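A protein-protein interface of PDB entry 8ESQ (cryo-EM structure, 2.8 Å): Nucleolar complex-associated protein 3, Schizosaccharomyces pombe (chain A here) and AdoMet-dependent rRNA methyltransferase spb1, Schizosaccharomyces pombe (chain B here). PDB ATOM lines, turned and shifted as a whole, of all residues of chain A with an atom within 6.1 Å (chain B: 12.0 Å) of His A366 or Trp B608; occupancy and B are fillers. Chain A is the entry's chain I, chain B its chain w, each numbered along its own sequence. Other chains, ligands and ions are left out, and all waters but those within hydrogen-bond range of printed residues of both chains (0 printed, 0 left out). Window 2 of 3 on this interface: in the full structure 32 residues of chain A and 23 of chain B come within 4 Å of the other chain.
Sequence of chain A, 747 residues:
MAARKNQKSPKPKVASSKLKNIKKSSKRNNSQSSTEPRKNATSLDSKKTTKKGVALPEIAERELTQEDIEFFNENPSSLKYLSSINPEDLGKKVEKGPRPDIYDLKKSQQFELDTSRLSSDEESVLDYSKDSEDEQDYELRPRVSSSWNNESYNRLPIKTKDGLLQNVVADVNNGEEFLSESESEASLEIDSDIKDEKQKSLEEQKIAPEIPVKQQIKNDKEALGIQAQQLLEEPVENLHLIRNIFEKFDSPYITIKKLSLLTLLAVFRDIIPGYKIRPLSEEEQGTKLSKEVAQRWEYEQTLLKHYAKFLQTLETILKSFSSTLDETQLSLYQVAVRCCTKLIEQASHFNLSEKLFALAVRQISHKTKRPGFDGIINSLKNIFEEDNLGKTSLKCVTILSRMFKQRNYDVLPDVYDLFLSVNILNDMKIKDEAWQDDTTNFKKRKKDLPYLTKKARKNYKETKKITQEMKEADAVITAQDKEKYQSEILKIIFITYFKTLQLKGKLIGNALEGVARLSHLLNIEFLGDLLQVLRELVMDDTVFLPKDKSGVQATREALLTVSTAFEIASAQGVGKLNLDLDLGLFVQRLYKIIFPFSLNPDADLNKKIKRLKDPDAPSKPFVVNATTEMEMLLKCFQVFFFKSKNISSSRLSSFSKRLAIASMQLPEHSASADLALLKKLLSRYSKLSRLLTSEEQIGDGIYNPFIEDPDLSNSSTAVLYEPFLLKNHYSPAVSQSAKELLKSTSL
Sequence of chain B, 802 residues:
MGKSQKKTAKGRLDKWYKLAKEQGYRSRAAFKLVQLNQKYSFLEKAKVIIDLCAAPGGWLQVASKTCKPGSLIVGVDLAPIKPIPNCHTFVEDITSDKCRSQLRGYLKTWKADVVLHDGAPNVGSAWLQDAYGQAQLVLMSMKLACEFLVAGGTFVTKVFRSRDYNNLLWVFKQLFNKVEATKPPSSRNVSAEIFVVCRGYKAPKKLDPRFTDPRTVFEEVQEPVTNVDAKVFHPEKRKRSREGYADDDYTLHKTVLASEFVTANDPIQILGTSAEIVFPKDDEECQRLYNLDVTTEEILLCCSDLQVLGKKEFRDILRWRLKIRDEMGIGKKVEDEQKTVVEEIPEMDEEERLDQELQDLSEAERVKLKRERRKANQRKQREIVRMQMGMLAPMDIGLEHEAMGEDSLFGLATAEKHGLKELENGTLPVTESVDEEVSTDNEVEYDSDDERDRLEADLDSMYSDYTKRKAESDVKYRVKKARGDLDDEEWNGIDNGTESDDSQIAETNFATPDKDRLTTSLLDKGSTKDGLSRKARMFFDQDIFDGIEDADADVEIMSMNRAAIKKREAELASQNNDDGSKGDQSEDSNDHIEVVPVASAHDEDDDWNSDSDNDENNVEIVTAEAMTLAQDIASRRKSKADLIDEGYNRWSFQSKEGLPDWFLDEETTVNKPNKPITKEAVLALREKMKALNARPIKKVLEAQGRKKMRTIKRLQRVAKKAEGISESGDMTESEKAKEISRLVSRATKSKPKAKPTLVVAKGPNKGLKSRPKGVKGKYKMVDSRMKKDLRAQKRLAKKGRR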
ATOM      1  N   VAL A 361       3.436 -11.868   9.060  1.00  0.00           N
ATOM      2  CA  VAL A 361       4.370 -10.805   9.419  1.00  0.00           C
ATOM      3  C   VAL A 361       4.386 -10.590  10.926  1.00  0.00           C
ATOM      4  O   VAL A 361       5.421 -10.221  11.497  1.00  0.00           O
ATOM      5  CB  VAL A 361       4.020  -9.513   8.656  1.00  0.00           C
ATOM      6  CG1 VAL A 361       4.969  -8.394   9.036  1.00  0.00           C
ATOM      7  CG2 VAL A 361       4.076  -9.757   7.157  1.00  0.00           C
ATOM      8  N   ARG A 362       3.256 -10.830  11.598  1.00  0.00           N
ATOM      9  CA  ARG A 362       3.217 -10.711  13.052  1.00  0.00           C
ATOM     10  C   ARG A 362       4.213 -11.650  13.719  1.00  0.00           C
ATOM     11  O   ARG A 362       4.781 -11.313  14.764  1.00  0.00           O
ATOM     12  CB  ARG A 362       1.803 -10.988  13.561  1.00  0.00           C
ATOM     13  CG  ARG A 362       1.599 -10.668  15.032  1.00  0.00           C
ATOM     14  CD  ARG A 362       0.187 -10.179  15.305  1.00  0.00           C
ATOM     15  NE  ARG A 362       0.029  -9.726  16.682  1.00  0.00           N
ATOM     16  CZ  ARG A 362      -1.040  -9.095  17.146  1.00  0.00           C
ATOM     17  NH1 ARG A 362      -2.071  -8.814  16.365  1.00  0.00           N
ATOM     18  NH2 ARG A 362      -1.077  -8.736  18.426  1.00  0.00           N
ATOM     19  N   GLN A 363       4.439 -12.828  13.133  1.00  0.00           N
ATOM     20  CA  GLN A 363       5.433 -13.744  13.683  1.00  0.00           C
ATOM     21  C   GLN A 363       6.846 -13.210  13.481  1.00  0.00           C
ATOM     22  O   GLN A 363       7.707 -13.371  14.353  1.00  0.00           O
ATOM     23  CB  GLN A 363       5.282 -15.123  13.043  1.00  0.00           C
ATOM     24  CG  GLN A 363       3.883 -15.709  13.152  1.00  0.00           C
ATOM     25  CD  GLN A 363       3.437 -15.906  14.589  1.00  0.00           C
ATOM     26  OE1 GLN A 363       4.246 -16.200  15.468  1.00  0.00           O
ATOM     27  NE2 GLN A 363       2.142 -15.743  14.833  1.00  0.00           N
ATOM     28  N   ILE A 364       7.103 -12.572  12.337  1.00  0.00           N
ATOM     29  CA  ILE A 364       8.430 -12.031  12.063  1.00  0.00           C
ATOM     30  C   ILE A 364       8.724 -10.776  12.874  1.00  0.00           C
ATOM     31  O   ILE A 364       9.891 -10.506  13.186  1.00  0.00           O
ATOM     32  CB  ILE A 364       8.592 -11.728  10.564  1.00  0.00           C
ATOM     33  CG1 ILE A 364       8.110 -12.907   9.722  1.00  0.00           C
ATOM     34  CG2 ILE A 364      10.042 -11.426  10.226  1.00  0.00           C
ATOM     35  CD1 ILE A 364       8.286 -12.691   8.239  1.00  0.00           C
ATOM     36  N   SER A 365       7.695 -10.009  13.244  1.00  0.00           N
ATOM     37  CA  SER A 365       7.911  -8.745  13.940  1.00  0.00           C
ATOM     38  C   SER A 365       8.520  -8.935  15.322  1.00  0.00           C
ATOM     39  O   SER A 365       8.971  -7.958  15.929  1.00  0.00           O
ATOM     40  CB  SER A 365       6.590  -7.983  14.061  1.00  0.00           C
ATOM     41  OG  SER A 365       5.654  -8.708  14.840  1.00  0.00           O
ATOM     42  N   HIS A 366       8.538 -10.162  15.831  1.00  0.00           N
ATOM     43  CA  HIS A 366       9.037 -10.418  17.170  1.00  0.00           C
ATOM     44  C   HIS A 366      10.557 -10.278  17.216  1.00  0.00           C
ATOM     45  O   HIS A 366      11.249 -10.349  16.196  1.00  0.00           O
ATOM     46  CB  HIS A 366       8.605 -11.808  17.627  1.00  0.00           C
ATOM     47  CG  HIS A 366       7.212 -11.847  18.172  1.00  0.00           C
ATOM     48  ND1 HIS A 366       6.702 -10.859  18.984  1.00  0.00           N
ATOM     49  CD2 HIS A 366       6.207 -12.733  17.982  1.00  0.00           C
ATOM     50  CE1 HIS A 366       5.450 -11.148  19.294  1.00  0.00           C
ATOM     51  NE2 HIS A 366       5.127 -12.282  18.700  1.00  0.00           N
ATOM     52  N   LYS A 367      11.073 -10.064  18.430  1.00  0.00           N
ATOM     53  CA  LYS A 367      12.499  -9.799  18.599  1.00  0.00           C
ATOM     54  C   LYS A 367      13.348 -11.003  18.211  1.00  0.00           C
ATOM     55  O   LYS A 367      14.410 -10.849  17.597  1.00  0.00           O
ATOM     56  CB  LYS A 367      12.787  -9.385  20.042  1.00  0.00           C
ATOM     57  CG  LYS A 367      11.883  -8.282  20.565  1.00  0.00           C
ATOM     58  CD  LYS A 367      12.095  -8.054  22.053  1.00  0.00           C
ATOM     59  CE  LYS A 367      11.145  -6.996  22.590  1.00  0.00           C
ATOM     60  NZ  LYS A 367      11.406  -6.693  24.024  1.00  0.00           N
ATOM     61  N   THR A 368      12.908 -12.205  18.565  1.00  0.00           N
ATOM     62  CA  THR A 368      13.674 -13.417  18.314  1.00  0.00           C
ATOM     63  C   THR A 368      13.131 -14.155  17.096  1.00  0.00           C
ATOM     64  O   THR A 368      11.948 -14.059  16.762  1.00  0.00           O
ATOM     65  CB  THR A 368      13.646 -14.343  19.532  1.00  0.00           C
ATOM     66  OG1 THR A 368      12.288 -14.636  19.881  1.00  0.00           O
ATOM     67  CG2 THR A 368      14.338 -13.682  20.714  1.00  0.00           C
ATOM     68  N   LYS A 369      14.016 -14.896  16.434  1.00  0.00           N
ATOM     69  CA  LYS A 369      13.648 -15.671  15.251  1.00  0.00           C
ATOM     70  C   LYS A 369      12.805 -16.863  15.683  1.00  0.00           C
ATOM     71  O   LYS A 369      13.332 -17.874  16.153  1.00  0.00           O
ATOM     72  CB  LYS A 369      14.894 -16.128  14.502  1.00  0.00           C
ATOM     73  CG  LYS A 369      15.702 -15.005  13.878  1.00  0.00           C
ATOM     74  CD  LYS A 369      16.749 -15.550  12.920  1.00  0.00           C
ATOM     75  CE  LYS A 369      17.485 -14.429  12.206  1.00  0.00           C
ATOM     76  NZ  LYS A 369      18.549 -14.950  11.302  1.00  0.00           N
ATOM     77  N   ARG A 370      11.492 -16.751  15.523  1.00  0.00           N
ATOM     78  CA  ARG A 370      10.603 -17.860  15.821  1.00  0.00           C
ATOM     79  C   ARG A 370      10.749 -18.952  14.765  1.00  0.00           C
ATOM     80  O   ARG A 370      11.175 -18.685  13.638  1.00  0.00           O
ATOM     81  CB  ARG A 370       9.160 -17.370  15.896  1.00  0.00           C
ATOM     82  CG  ARG A 370       8.872 -16.506  17.113  1.00  0.00           C
ATOM     83  CD  ARG A 370       7.379 -16.289  17.299  1.00  0.00           C
ATOM     84  NE  ARG A 370       7.066 -15.807  18.639  1.00  0.00           N
ATOM     85  CZ  ARG A 370       5.838 -15.585  19.088  1.00  0.00           C
ATOM     86  NH1 ARG A 370       4.775 -15.786  18.326  1.00  0.00           N
ATOM     87  NH2 ARG A 370       5.671 -15.147  20.334  1.00  0.00           N
ATOM     88  N   GLN A 406       5.148  -0.140  14.583  1.00  0.00           N
ATOM     89  CA  GLN A 406       4.854  -0.821  15.839  1.00  0.00           C
ATOM     90  C   GLN A 406       6.135  -1.184  16.580  1.00  0.00           C
ATOM     91  O   GLN A 406       6.200  -1.082  17.811  1.00  0.00           O
ATOM     92  CB  GLN A 406       4.015  -2.069  15.575  1.00  0.00           C
ATOM     93  CG  GLN A 406       2.552  -1.785  15.278  1.00  0.00           C
ATOM     94  CD  GLN A 406       1.696  -3.036  15.313  1.00  0.00           C
ATOM     95  OE1 GLN A 406       2.186  -4.129  15.596  1.00  0.00           O
ATOM     96  NE2 GLN A 406       0.410  -2.883  15.024  1.00  0.00           N
ATOM     97  N   ARG A 407       7.160  -1.610  15.849  1.00  0.00           N
ATOM     98  CA  ARG A 407       8.439  -1.981  16.436  1.00  0.00           C
ATOM     99  C   ARG A 407       9.401  -0.808  16.555  1.00  0.00           C
ATOM    100  O   ARG A 407      10.554  -1.014  16.948  1.00  0.00           O
ATOM    101  CB  ARG A 407       9.094  -3.095  15.613  1.00  0.00           C
ATOM    102  CG  ARG A 407       8.338  -4.408  15.647  1.00  0.00           C
ATOM    103  CD  ARG A 407       7.903  -4.739  17.061  1.00  0.00           C
ATOM    104  NE  ARG A 407       7.726  -6.172  17.261  1.00  0.00           N
ATOM    105  CZ  ARG A 407       7.093  -6.706  18.295  1.00  0.00           C
ATOM    106  NH1 ARG A 407       6.559  -5.953  19.241  1.00  0.00           N
ATOM    107  NH2 ARG A 407       6.987  -8.029  18.377  1.00  0.00           N
ATOM    108  N   VAL A 411      13.749  -4.171  14.024  1.00  0.00           N
ATOM    109  CA  VAL A 411      13.460  -5.538  13.616  1.00  0.00           C
ATOM    110  C   VAL A 411      14.761  -6.206  13.190  1.00  0.00           C
ATOM    111  O   VAL A 411      15.828  -5.589  13.170  1.00  0.00           O
ATOM    112  CB  VAL A 411      12.425  -5.604  12.473  1.00  0.00           C
ATOM    113  CG1 VAL A 411      11.031  -5.302  12.999  1.00  0.00           C
ATOM    114  CG2 VAL A 411      12.807  -4.644  11.362  1.00  0.00           C
ATOM    115  N   LEU A 412      14.658  -7.487  12.851  1.00  0.00           N
ATOM    116  CA  LEU A 412      15.824  -8.245  12.430  1.00  0.00           C
ATOM    117  C   LEU A 412      16.368  -7.698  11.111  1.00  0.00           C
ATOM    118  O   LEU A 412      15.606  -7.231  10.261  1.00  0.00           O
ATOM    119  CB  LEU A 412      15.467  -9.720  12.281  1.00  0.00           C
ATOM    120  CG  LEU A 412      14.736 -10.307  13.486  1.00  0.00           C
ATOM    121  CD1 LEU A 412      14.343 -11.748  13.229  1.00  0.00           C
ATOM    122  CD2 LEU A 412      15.614 -10.200  14.722  1.00  0.00           C
ATOM    123  N   TRP B 608       0.252  -6.774  22.006  1.00  0.00           N
ATOM    124  CA  TRP B 608       1.269  -5.735  21.887  1.00  0.00           C
ATOM    125  C   TRP B 608       1.750  -5.608  20.444  1.00  0.00           C
ATOM    126  O   TRP B 608       2.785  -4.999  20.173  1.00  0.00           O
ATOM    127  CB  TRP B 608       2.442  -6.017  22.835  1.00  0.00           C
ATOM    128  CG  TRP B 608       3.149  -7.328  22.610  1.00  0.00           C
ATOM    129  CD1 TRP B 608       2.588  -8.573  22.588  1.00  0.00           C
ATOM    130  CD2 TRP B 608       4.559  -7.523  22.429  1.00  0.00           C
ATOM    131  NE1 TRP B 608       3.555  -9.525  22.377  1.00  0.00           N
ATOM    132  CE2 TRP B 608       4.773  -8.907  22.279  1.00  0.00           C
ATOM    133  CE3 TRP B 608       5.658  -6.660  22.368  1.00  0.00           C
ATOM    134  CZ2 TRP B 608       6.041  -9.448  22.073  1.00  0.00           C
ATOM    135  CZ3 TRP B 608       6.916  -7.199  22.163  1.00  0.00           C
ATOM    136  CH2 TRP B 608       7.096  -8.580  22.016  1.00  0.00           C
ATOM    137  N   ASN B 609       0.984  -6.197  19.520  1.00  0.00           N
ATOM    138  CA  ASN B 609       1.232  -6.057  18.090  1.00  0.00           C
ATOM    139  C   ASN B 609      -0.073  -5.924  17.313  1.00  0.00           C
ATOM    140  O   ASN B 609      -0.125  -6.253  16.122  1.00  0.00           O
ATOM    141  CB  ASN B 609       2.045  -7.236  17.552  1.00  0.00           C
ATOM    142  CG  ASN B 609       3.503  -7.170  17.956  1.00  0.00           C
ATOM    143  OD1 ASN B 609       4.271  -6.379  17.411  1.00  0.00           O
ATOM    144  ND2 ASN B 609       3.890  -8.002  18.915  1.00  0.00           N
ATOM    145  N   SER B 610      -1.129  -5.448  17.966  1.00  0.00           N
ATOM    146  CA  SER B 610      -2.442  -5.388  17.337  1.00  0.00           C
ATOM    147  C   SER B 610      -2.470  -4.331  16.239  1.00  0.00           C
ATOM    148  O   SER B 610      -2.031  -3.195  16.442  1.00  0.00           O
ATOM    149  CB  SER B 610      -3.513  -5.085  18.384  1.00  0.00           C
ATOM    150  OG  SER B 610      -3.324  -3.799  18.947  1.00  0.00           O
ATOM    151  N   ASP B 611      -2.983  -4.712  15.076  1.00  0.00           N
ATOM    152  CA  ASP B 611      -3.154  -3.797  13.945  1.00  0.00           C
ATOM    153  C   ASP B 611      -4.555  -3.201  13.918  1.00  0.00           C
ATOM    154  O   ASP B 611      -5.276  -3.300  12.925  1.00  0.00           O
ATOM    155  CB  ASP B 611      -2.838  -4.513  12.639  1.00  0.00           C
ATOM    156  CG  ASP B 611      -1.352  -4.653  12.405  1.00  0.00           C
ATOM    157  OD1 ASP B 611      -0.590  -3.849  12.980  1.00  0.00           O
ATOM    158  OD2 ASP B 611      -0.946  -5.562  11.650  1.00  0.00           O
ATOM    159  N   SER B 612      -4.956  -2.567  15.021  1.00  0.00           N
ATOM    160  CA  SER B 612      -6.274  -1.950  15.104  1.00  0.00           C
ATOM    161  C   SER B 612      -6.384  -0.672  14.285  1.00  0.00           C
ATOM    162  O   SER B 612      -7.493  -0.144  14.141  1.00  0.00           O
ATOM    163  CB  SER B 612      -6.623  -1.656  16.564  1.00  0.00           C
ATOM    164  OG  SER B 612      -5.712  -0.731  17.129  1.00  0.00           O
ATOM    165  N   ASP B 613      -5.276  -0.161  13.754  1.00  0.00           N
ATOM    166  CA  ASP B 613      -5.290   1.063  12.962  1.00  0.00           C
ATOM    167  C   ASP B 613      -6.106   0.890  11.684  1.00  0.00           C
ATOM    168  O   ASP B 613      -6.320  -0.229  11.219  1.00  0.00           O
ATOM    169  CB  ASP B 613      -3.862   1.491  12.614  1.00  0.00           C
ATOM    170  CG  ASP B 613      -3.025   0.347  12.075  1.00  0.00           C
ATOM    171  OD1 ASP B 613      -3.498  -0.809  12.117  1.00  0.00           O
ATOM    172  OD2 ASP B 613      -1.895   0.603  11.609  1.00  0.00           O
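The guanidinium group of Arg A362 sits close to the backbone carbonyl oxygen of Asn B609 (3.2 Å). The side-chain amide oxygen of Gln A406 sits close to the backbone carbonyl oxygen of Asn B609, 3.2 Å away. The backbone carbonyl oxygen of Ser B610 sits at hydrogen-bond distance from the side-chain amide nitrogen of Gln A406 (2.8 Å). NE2 of Gln A406 is in hydrogen-bond range of OD1 of Asp B611 (2.5 Å). The side-chain amide oxygen (OD1) of Asn B609 lies within hydrogen-bond range of the guanidinium group (NH1) of Arg A407 (3.0 Å). NH2 of Arg A362 sits close to N of Ser B610 (3.3 Å).
The side-chain hydroxyl (OG) of Ser A365 sits at hydrogen-bond distance from the backbone carbonyl oxygen (O) of Arg A362, at 2.7 Å. The guanidinium group of Arg A407 is in hydrogen-bond range of the backbone carbonyl oxygen of Ser A365, at 2.6 Å. A ring nitrogen (NE2) of His A366 sits at hydrogen-bond distance from the guanidinium group of Arg A370 (3.3 Å). The guanidinium group of Arg A407 lies within hydrogen-bond range of a ring nitrogen (ND1) of His A366 (2.9 Å).
Among the printed residues, pairs that only touch across the chains: Ser A365 with Asn B609, His A366 with Trp B608, His A366 with Asn B609 and Arg A407 with Trp B608.
His A366 touches two residues of chain B. Arg A362 touches just these residues of chain B: Asn B609 and Ser B610. Of chain B, only Asn B609 comes within 4 Å of Ser A365. No residue of chain B comes within 4 Å of Lys A367. No residue of chain B comes within 4 Å of Thr A368. No residue of chain B comes within 4 Å of Val A411. Of the printed residues of chain A, Asn B609 touches Arg A362 (3.2 Å), Ser A365 (3.7 Å), His A366 (3.5 Å), Gln A406 (3.2 Å) and Arg A407 (3.0 Å). Printed residues of chain A within 4 Å of Asp B611: Gln A406. Of the printed residues of chain A, Ser B610 touches Arg A362 and Gln A406. Printed residues of chain B within 4 Å of Arg A407: Trp B608 (3.2 Å) and Asn B609 (3.0 Å). The nearest residue of chain B that does not touch His A366 is Ser B610 (8.8 Å).
Printed residues of chain B that touch a printed residue of chain A: Trp B608, Asn B609, Ser B610 and Asp B611. Hydrophobic or aromatic side chains of chain B that line the printed part of chain A: Trp B608. Hydrophobic or aromatic side chains of chain A within 4 Å of the printed part of chain B: His A366.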
